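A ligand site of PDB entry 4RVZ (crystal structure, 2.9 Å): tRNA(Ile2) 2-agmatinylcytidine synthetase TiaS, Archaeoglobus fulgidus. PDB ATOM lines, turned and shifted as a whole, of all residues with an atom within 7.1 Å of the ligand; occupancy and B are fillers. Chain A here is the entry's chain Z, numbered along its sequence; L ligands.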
ATOM      1  N   ARG A  44     -16.014 -11.687  31.885  1.00  0.00           N
ATOM      2  CA  ARG A  44     -16.969 -11.852  33.003  1.00  0.00           C
ATOM      3  C   ARG A  44     -16.469 -12.800  34.087  1.00  0.00           C
ATOM      4  O   ARG A  44     -15.824 -13.825  33.827  1.00  0.00           O
ATOM      5  CB  ARG A  44     -18.339 -12.341  32.515  1.00  0.00           C
ATOM      6  CG  ARG A  44     -19.049 -11.400  31.570  1.00  0.00           C
ATOM      7  CD  ARG A  44     -19.209 -10.015  32.180  1.00  0.00           C
ATOM      8  NE  ARG A  44     -19.396  -9.003  31.145  1.00  0.00           N
ATOM      9  CZ  ARG A  44     -20.453  -8.204  31.041  1.00  0.00           C
ATOM     10  NH1 ARG A  44     -21.435  -8.282  31.925  1.00  0.00           N
ATOM     11  NH2 ARG A  44     -20.523  -7.333  30.040  1.00  0.00           N
ATOM     12  N   ARG A  54     -23.987  -3.932  38.125  1.00  0.00           N
ATOM     13  CA  ARG A  54     -24.597  -5.040  37.379  1.00  0.00           C
ATOM     14  C   ARG A  54     -23.600  -5.769  36.458  1.00  0.00           C
ATOM     15  O   ARG A  54     -22.876  -5.123  35.699  1.00  0.00           O
ATOM     16  CB  ARG A  54     -25.775  -4.524  36.539  1.00  0.00           C
ATOM     17  CG  ARG A  54     -26.530  -5.592  35.766  1.00  0.00           C
ATOM     18  CD  ARG A  54     -26.830  -5.143  34.344  1.00  0.00           C
ATOM     19  NE  ARG A  54     -25.672  -5.307  33.464  1.00  0.00           N
ATOM     20  CZ  ARG A  54     -25.436  -4.553  32.387  1.00  0.00           C
ATOM     21  NH1 ARG A  54     -26.272  -3.580  32.064  1.00  0.00           N
ATOM     22  NH2 ARG A  54     -24.362  -4.774  31.643  1.00  0.00           N
ATOM     23  N   GLU A 159     -18.489  -9.778  21.402  1.00  0.00           N
ATOM     24  CA  GLU A 159     -19.489  -8.737  21.549  1.00  0.00           C
ATOM     25  C   GLU A 159     -18.995  -7.437  20.967  1.00  0.00           C
ATOM     26  O   GLU A 159     -17.955  -6.919  21.351  1.00  0.00           O
ATOM     27  CB  GLU A 159     -19.921  -8.537  23.001  1.00  0.00           C
ATOM     28  CG  GLU A 159     -21.189  -7.680  23.119  1.00  0.00           C
ATOM     29  CD  GLU A 159     -21.857  -7.812  24.472  1.00  0.00           C
ATOM     30  OE1 GLU A 159     -21.293  -8.528  25.328  1.00  0.00           O
ATOM     31  OE2 GLU A 159     -22.929  -7.205  24.685  1.00  0.00           O
ATOM     32  N   ILE A 161     -19.470  -3.925  21.141  1.00  0.00           N
ATOM     33  CA  ILE A 161     -20.071  -2.870  21.952  1.00  0.00           C
ATOM     34  C   ILE A 161     -20.089  -1.543  21.191  1.00  0.00           C
ATOM     35  O   ILE A 161     -19.084  -1.136  20.620  1.00  0.00           O
ATOM     36  CB  ILE A 161     -19.325  -2.680  23.284  1.00  0.00           C
ATOM     37  CG1 ILE A 161     -19.063  -4.027  23.987  1.00  0.00           C
ATOM     38  CG2 ILE A 161     -20.117  -1.733  24.159  1.00  0.00           C
ATOM     39  CD1 ILE A 161     -20.199  -4.502  24.909  1.00  0.00           C
ATOM     40  N   PHE A 192     -26.279 -14.398  18.130  1.00  0.00           N
ATOM     41  CA  PHE A 192     -27.252 -14.929  19.082  1.00  0.00           C
ATOM     42  C   PHE A 192     -27.566 -13.958  20.220  1.00  0.00           C
ATOM     43  O   PHE A 192     -26.803 -13.042  20.493  1.00  0.00           O
ATOM     44  CB  PHE A 192     -26.689 -16.204  19.680  1.00  0.00           C
ATOM     45  CG  PHE A 192     -25.439 -15.991  20.457  1.00  0.00           C
ATOM     46  CD1 PHE A 192     -25.445 -16.051  21.834  1.00  0.00           C
ATOM     47  CD2 PHE A 192     -24.235 -15.718  19.813  1.00  0.00           C
ATOM     48  CE1 PHE A 192     -24.289 -15.849  22.571  1.00  0.00           C
ATOM     49  CE2 PHE A 192     -23.070 -15.503  20.531  1.00  0.00           C
ATOM     50  CZ  PHE A 192     -23.097 -15.568  21.910  1.00  0.00           C
ATOM     51  N   ASP A 193     -28.698 -14.200  20.882  1.00  0.00           N
ATOM     52  CA  ASP A 193     -29.037 -13.543  22.155  1.00  0.00           C
ATOM     53  C   ASP A 193     -29.022 -12.033  22.149  1.00  0.00           C
ATOM     54  O   ASP A 193     -28.556 -11.407  23.095  1.00  0.00           O
ATOM     55  CB  ASP A 193     -28.134 -14.038  23.292  1.00  0.00           C
ATOM     56  CG  ASP A 193     -28.588 -15.360  23.882  1.00  0.00           C
ATOM     57  OD1 ASP A 193     -29.777 -15.709  23.720  1.00  0.00           O
ATOM     58  OD2 ASP A 193     -27.757 -16.039  24.513  1.00  0.00           O
ATOM     59  N   ASN A 194     -29.550 -11.442  21.081  1.00  0.00           N
ATOM     60  CA  ASN A 194     -29.575  -9.997  20.947  1.00  0.00           C
ATOM     61  C   ASN A 194     -31.004  -9.496  20.904  1.00  0.00           C
ATOM     62  O   ASN A 194     -31.251  -8.326  20.643  1.00  0.00           O
ATOM     63  CB  ASN A 194     -28.842  -9.605  19.679  1.00  0.00           C
ATOM     64  CG  ASN A 194     -27.383  -9.986  19.719  1.00  0.00           C
ATOM     65  OD1 ASN A 194     -26.725  -9.795  20.749  1.00  0.00           O
ATOM     66  ND2 ASN A 194     -26.871 -10.538  18.627  1.00  0.00           N
ATOM     67  N   VAL A 195     -31.923 -10.398  21.179  1.00  0.00           N
ATOM     68  CA  VAL A 195     -33.348 -10.095  21.121  1.00  0.00           C
ATOM     69  C   VAL A 195     -34.150 -11.308  21.560  1.00  0.00           C
ATOM     70  O   VAL A 195     -33.776 -12.462  21.307  1.00  0.00           O
ATOM     71  CB  VAL A 195     -33.777  -9.631  19.715  1.00  0.00           C
ATOM     72  CG1 VAL A 195     -33.955 -10.786  18.755  1.00  0.00           C
ATOM     73  CG2 VAL A 195     -35.026  -8.815  19.807  1.00  0.00           C
ATOM     74  N   VAL A 202     -36.040  -6.183  22.932  1.00  0.00           N
ATOM     75  CA  VAL A 202     -34.687  -6.217  22.405  1.00  0.00           C
ATOM     76  C   VAL A 202     -33.730  -6.278  23.574  1.00  0.00           C
ATOM     77  O   VAL A 202     -33.777  -5.463  24.495  1.00  0.00           O
ATOM     78  CB  VAL A 202     -34.372  -4.996  21.545  1.00  0.00           C
ATOM     79  CG1 VAL A 202     -32.968  -5.118  20.942  1.00  0.00           C
ATOM     80  CG2 VAL A 202     -35.421  -4.822  20.477  1.00  0.00           C
ATOM     81  N   VAL A 203     -32.844  -7.265  23.526  1.00  0.00           N
ATOM     82  CA  VAL A 203     -32.074  -7.660  24.683  1.00  0.00           C
ATOM     83  C   VAL A 203     -30.734  -6.921  24.795  1.00  0.00           C
ATOM     84  O   VAL A 203     -30.245  -6.656  25.897  1.00  0.00           O
ATOM     85  CB  VAL A 203     -31.891  -9.200  24.668  1.00  0.00           C
ATOM     86  CG1 VAL A 203     -30.773  -9.654  25.569  1.00  0.00           C
ATOM     87  CG2 VAL A 203     -33.204  -9.880  25.054  1.00  0.00           C
ATOM     88  N   CYS A 204     -30.164  -6.543  23.646  1.00  0.00           N
ATOM     89  CA  CYS A 204     -28.805  -6.034  23.604  1.00  0.00           C
ATOM     90  C   CYS A 204     -28.692  -4.530  23.949  1.00  0.00           C
ATOM     91  O   CYS A 204     -27.702  -3.877  23.631  1.00  0.00           O
ATOM     92  CB  CYS A 204     -28.175  -6.346  22.244  1.00  0.00           C
ATOM     93  SG  CYS A 204     -29.253  -5.977  20.847  1.00  0.00           S
ATOM     94  N   ILE A 205     -29.708  -4.009  24.623  1.00  0.00           N
ATOM     95  CA  ILE A 205     -29.754  -2.597  24.936  1.00  0.00           C
ATOM     96  C   ILE A 205     -30.073  -2.375  26.406  1.00  0.00           C
ATOM     97  O   ILE A 205     -31.092  -2.824  26.904  1.00  0.00           O
ATOM     98  CB  ILE A 205     -30.800  -1.907  24.081  1.00  0.00           C
ATOM     99  CG1 ILE A 205     -30.381  -1.985  22.614  1.00  0.00           C
ATOM    100  CG2 ILE A 205     -30.986  -0.466  24.532  1.00  0.00           C
ATOM    101  CD1 ILE A 205     -31.391  -1.436  21.659  1.00  0.00           C
ATOM    102  N   PRO A 206     -29.180  -1.668  27.103  1.00  0.00           N
ATOM    103  CA  PRO A 206     -29.344  -1.412  28.546  1.00  0.00           C
ATOM    104  C   PRO A 206     -30.341  -0.305  28.891  1.00  0.00           C
ATOM    105  O   PRO A 206     -30.556   0.625  28.122  1.00  0.00           O
ATOM    106  CB  PRO A 206     -27.938  -1.015  28.990  1.00  0.00           C
ATOM    107  CG  PRO A 206     -27.294  -0.477  27.770  1.00  0.00           C
ATOM    108  CD  PRO A 206     -27.860  -1.229  26.614  1.00  0.00           C
ATOM    109  N   TYR A 214     -25.655  -0.254  22.256  1.00  0.00           N
ATOM    110  CA  TYR A 214     -25.876  -1.678  22.154  1.00  0.00           C
ATOM    111  C   TYR A 214     -24.578  -2.459  22.253  1.00  0.00           C
ATOM    112  O   TYR A 214     -23.538  -2.007  21.805  1.00  0.00           O
ATOM    113  CB  TYR A 214     -26.617  -2.056  20.851  1.00  0.00           C
ATOM    114  CG  TYR A 214     -25.943  -1.652  19.545  1.00  0.00           C
ATOM    115  CD1 TYR A 214     -26.429  -0.580  18.800  1.00  0.00           C
ATOM    116  CD2 TYR A 214     -24.850  -2.347  19.028  1.00  0.00           C
ATOM    117  CE1 TYR A 214     -25.838  -0.193  17.597  1.00  0.00           C
ATOM    118  CE2 TYR A 214     -24.252  -1.983  17.829  1.00  0.00           C
ATOM    119  CZ  TYR A 214     -24.760  -0.893  17.114  1.00  0.00           C
ATOM    120  OH  TYR A 214     -24.186  -0.493  15.918  1.00  0.00           O
ATOM    121  N   GLY A 215     -24.674  -3.644  22.853  1.00  0.00           N
ATOM    122  CA  GLY A 215     -23.603  -4.629  22.795  1.00  0.00           C
ATOM    123  C   GLY A 215     -24.130  -5.892  22.127  1.00  0.00           C
ATOM    124  O   GLY A 215     -24.910  -6.642  22.718  1.00  0.00           O
ATOM    125  N   ILE A 216     -23.697  -6.128  20.897  1.00  0.00           N
ATOM    126  CA  ILE A 216     -24.185  -7.240  20.097  1.00  0.00           C
ATOM    127  C   ILE A 216     -23.287  -8.480  20.163  1.00  0.00           C
ATOM    128  O   ILE A 216     -22.106  -8.400  19.847  1.00  0.00           O
ATOM    129  CB  ILE A 216     -24.361  -6.811  18.638  1.00  0.00           C
ATOM    130  CG1 ILE A 216     -25.588  -5.920  18.495  1.00  0.00           C
ATOM    131  CG2 ILE A 216     -24.455  -8.033  17.739  1.00  0.00           C
ATOM    132  CD1 ILE A 216     -25.810  -5.424  17.105  1.00  0.00           C
ATOM    133  N   ARG A 217     -23.851  -9.617  20.583  1.00  0.00           N
ATOM    134  CA  ARG A 217     -23.088 -10.870  20.658  1.00  0.00           C
ATOM    135  C   ARG A 217     -23.180 -11.761  19.412  1.00  0.00           C
ATOM    136  O   ARG A 217     -24.225 -11.877  18.776  1.00  0.00           O
ATOM    137  CB  ARG A 217     -23.488 -11.677  21.885  1.00  0.00           C
ATOM    138  CG  ARG A 217     -22.804 -11.289  23.158  1.00  0.00           C
ATOM    139  CD  ARG A 217     -23.842 -10.952  24.204  1.00  0.00           C
ATOM    140  NE  ARG A 217     -23.300 -11.007  25.562  1.00  0.00           N
ATOM    141  CZ  ARG A 217     -24.055 -10.946  26.649  1.00  0.00           C
ATOM    142  NH1 ARG A 217     -25.366 -10.815  26.542  1.00  0.00           N
ATOM    143  NH2 ARG A 217     -23.487 -11.010  27.852  1.00  0.00           N
ATOM    144  N   PRO A 397     -35.598 -17.873  28.752  1.00  0.00           N
ATOM    145  CA  PRO A 397     -35.683 -17.025  27.557  1.00  0.00           C
ATOM    146  C   PRO A 397     -34.540 -16.022  27.558  1.00  0.00           C
ATOM    147  O   PRO A 397     -34.062 -15.662  28.626  1.00  0.00           O
ATOM    148  CB  PRO A 397     -37.007 -16.292  27.755  1.00  0.00           C
ATOM    149  CG  PRO A 397     -37.139 -16.201  29.239  1.00  0.00           C
ATOM    150  CD  PRO A 397     -36.637 -17.521  29.740  1.00  0.00           C
ATOM    151  N   PRO A 398     -34.103 -15.569  26.360  1.00  0.00           N
ATOM    152  CA  PRO A 398     -32.905 -14.724  26.263  1.00  0.00           C
ATOM    153  C   PRO A 398     -32.922 -13.463  27.150  1.00  0.00           C
ATOM    154  O   PRO A 398     -31.868 -13.034  27.622  1.00  0.00           O
ATOM    155  CB  PRO A 398     -32.850 -14.363  24.776  1.00  0.00           C
ATOM    156  CG  PRO A 398     -33.645 -15.411  24.089  1.00  0.00           C
ATOM    157  CD  PRO A 398     -34.725 -15.793  25.050  1.00  0.00           C
ATOM    158  N   SER A 399     -34.093 -12.887  27.413  1.00  0.00           N
ATOM    159  CA  SER A 399     -34.160 -11.716  28.282  1.00  0.00           C
ATOM    160  C   SER A 399     -33.915 -12.056  29.746  1.00  0.00           C
ATOM    161  O   SER A 399     -33.920 -11.174  30.615  1.00  0.00           O
ATOM    162  CB  SER A 399     -35.491 -10.974  28.114  1.00  0.00           C
ATOM    163  OG  SER A 399     -36.593 -11.829  28.371  1.00  0.00           O
ATOM    164  N   ALA A 400     -33.704 -13.340  30.032  1.00  0.00           N
ATOM    165  CA  ALA A 400     -33.410 -13.789  31.382  1.00  0.00           C
ATOM    166  C   ALA A 400     -32.055 -14.474  31.425  1.00  0.00           C
ATOM    167  O   ALA A 400     -31.687 -15.040  32.454  1.00  0.00           O
ATOM    168  CB  ALA A 400     -34.483 -14.721  31.875  1.00  0.00           C
ATOM    169  N   ARG A 401     -31.341 -14.432  30.302  1.00  0.00           N
ATOM    170  CA  ARG A 401     -30.024 -15.080  30.194  1.00  0.00           C
ATOM    171  C   ARG A 401     -28.968 -14.317  30.974  1.00  0.00           C
ATOM    172  O   ARG A 401     -28.826 -13.098  30.830  1.00  0.00           O
ATOM    173  CB  ARG A 401     -29.612 -15.186  28.720  1.00  0.00           C
ATOM    174  CG  ARG A 401     -28.288 -15.904  28.464  1.00  0.00           C
ATOM    175  CD  ARG A 401     -28.450 -17.057  27.481  1.00  0.00           C
ATOM    176  NE  ARG A 401     -29.607 -17.883  27.840  1.00  0.00           N
ATOM    177  CZ  ARG A 401     -30.676 -18.075  27.070  1.00  0.00           C
ATOM    178  NH1 ARG A 401     -30.739 -17.556  25.859  1.00  0.00           N
ATOM    179  NH2 ARG A 401     -31.665 -18.825  27.517  1.00  0.00           N
ATOM    180  N   ARG A 402     -28.215 -15.048  31.804  1.00  0.00           N
ATOM    181  CA  ARG A 402     -27.080 -14.454  32.511  1.00  0.00           C
ATOM    182  C   ARG A 402     -25.858 -14.457  31.604  1.00  0.00           C
ATOM    183  O   ARG A 402     -25.723 -15.332  30.756  1.00  0.00           O
ATOM    184  CB  ARG A 402     -26.797 -15.170  33.837  1.00  0.00           C
ATOM    185  CG  ARG A 402     -27.997 -15.200  34.773  1.00  0.00           C
ATOM    186  CD  ARG A 402     -27.642 -15.744  36.147  1.00  0.00           C
ATOM    187  NE  ARG A 402     -27.071 -14.720  37.012  1.00  0.00           N
ATOM    188  CZ  ARG A 402     -26.690 -14.927  38.280  1.00  0.00           C
ATOM    189  NH1 ARG A 402     -26.814 -16.132  38.816  1.00  0.00           N
ATOM    190  NH2 ARG A 402     -26.181 -13.933  38.989  1.00  0.00           N
ATOM    191  N   HIS A 403     -24.980 -13.481  31.790  1.00  0.00           N
ATOM    192  CA  HIS A 403     -23.831 -13.284  30.912  1.00  0.00           C
ATOM    193  C   HIS A 403     -23.037 -14.560  30.584  1.00  0.00           C
ATOM    194  O   HIS A 403     -22.666 -14.779  29.433  1.00  0.00           O
ATOM    195  CB  HIS A 403     -22.909 -12.206  31.490  1.00  0.00           C
ATOM    196  CG  HIS A 403     -23.625 -10.935  31.845  1.00  0.00           C
ATOM    197  ND1 HIS A 403     -23.836  -9.917  30.932  1.00  0.00           N
ATOM    198  CD2 HIS A 403     -24.187 -10.514  33.003  1.00  0.00           C
ATOM    199  CE1 HIS A 403     -24.479  -8.930  31.509  1.00  0.00           C
ATOM    200  NE2 HIS A 403     -24.705  -9.268  32.769  1.00  0.00           N
HETATM  201  N1  LIG L   1     -31.689  -7.927  32.835  1.00  0.00           N
HETATM  202  C1  LIG L   1     -31.855  -9.052  31.956  1.00  0.00           C
HETATM  203  C2  LIG L   1     -30.760  -9.454  31.028  1.00  0.00           C
HETATM  204  C3  LIG L   1     -31.032  -9.562  29.566  1.00  0.00           C
HETATM  205  C4  LIG L   1     -29.890  -9.933  28.682  1.00  0.00           C
HETATM  206  N2  LIG L   1     -28.859  -8.957  28.431  1.00  0.00           N
HETATM  207  C5  LIG L   1     -27.897  -9.141  27.389  1.00  0.00           C
HETATM  208  O1  LIG L   1     -27.938 -10.165  26.707  1.00  0.00           O
HETATM  209  C6  LIG L   1     -26.810  -8.120  27.120  1.00  0.00           C
HETATM  210  N3  LIG L   1     -26.368  -7.813  25.782  1.00  0.00           N
HETATM  211  N4  LIG L   1     -26.655  -8.584  24.868  1.00  0.00           N
HETATM  212  N5  LIG L   1     -26.918  -9.328  23.948  1.00  0.00           N
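OD1 of Asn 194 sits close to N5 of the ligand, at 3.2 Å.
The guanidinium group (NH1) of Arg 217 lies within hydrogen-bond range of an oxygen (O1) of the ligand, at 2.7 Å.
N of Val 203 is in hydrogen-bond range of O of Asn 194 (3.5 Å).
OE1 of Glu 159 lies within salt-bridge range of NE of Arg 217 (3.2 Å).
The backbone carbonyl oxygen (O) of Phe 192 sits at hydrogen-bond distance from the side-chain amide nitrogen (ND2) of Asn 194 (3.1 Å).
The backbone carbonyl oxygen (O) of Asn 194 is in hydrogen-bond range of the side-chain sulfur (SG) of Cys 204 (3.1 Å).
The backbone carbonyl oxygen (O) of Arg 217 is in hydrogen-bond range of the backbone NH (N) of Phe 192, at 3.3 Å.
The guanidinium group (NH1) of Arg 401 lies within salt-bridge range of the side-chain carboxylate (OD1) of Asp 193.
ND1 of His 403 is in hydrogen-bond range of NH2 of Arg 217 (3.3 Å).
The backbone carbonyl oxygen (O) of Cys 204 sits at hydrogen-bond distance from the backbone NH (N) of Gly 215 (3.1 Å).
The backbone carbonyl oxygen (O) of Asp 193 sits close to a nitrogen (N5) of the ligand (2.8 Å).
O of Gly 215 lies close to N4 of the ligand.
Glu 159 touches the ligand.
Val 203 touches the ligand.
Cys 204 touches the ligand.
Pro 398 touches the ligand (O to C4, 3.8 Å).
Ser 399 touches the ligand.
O of Arg 401 touches C4 of the ligand, 3.97 Å away.
Hydrophobic or aromatic side chains within 4 Å of the ligand: Val 203.
Of the 24 residues printed, 10 come within 4 Å of the ligand.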
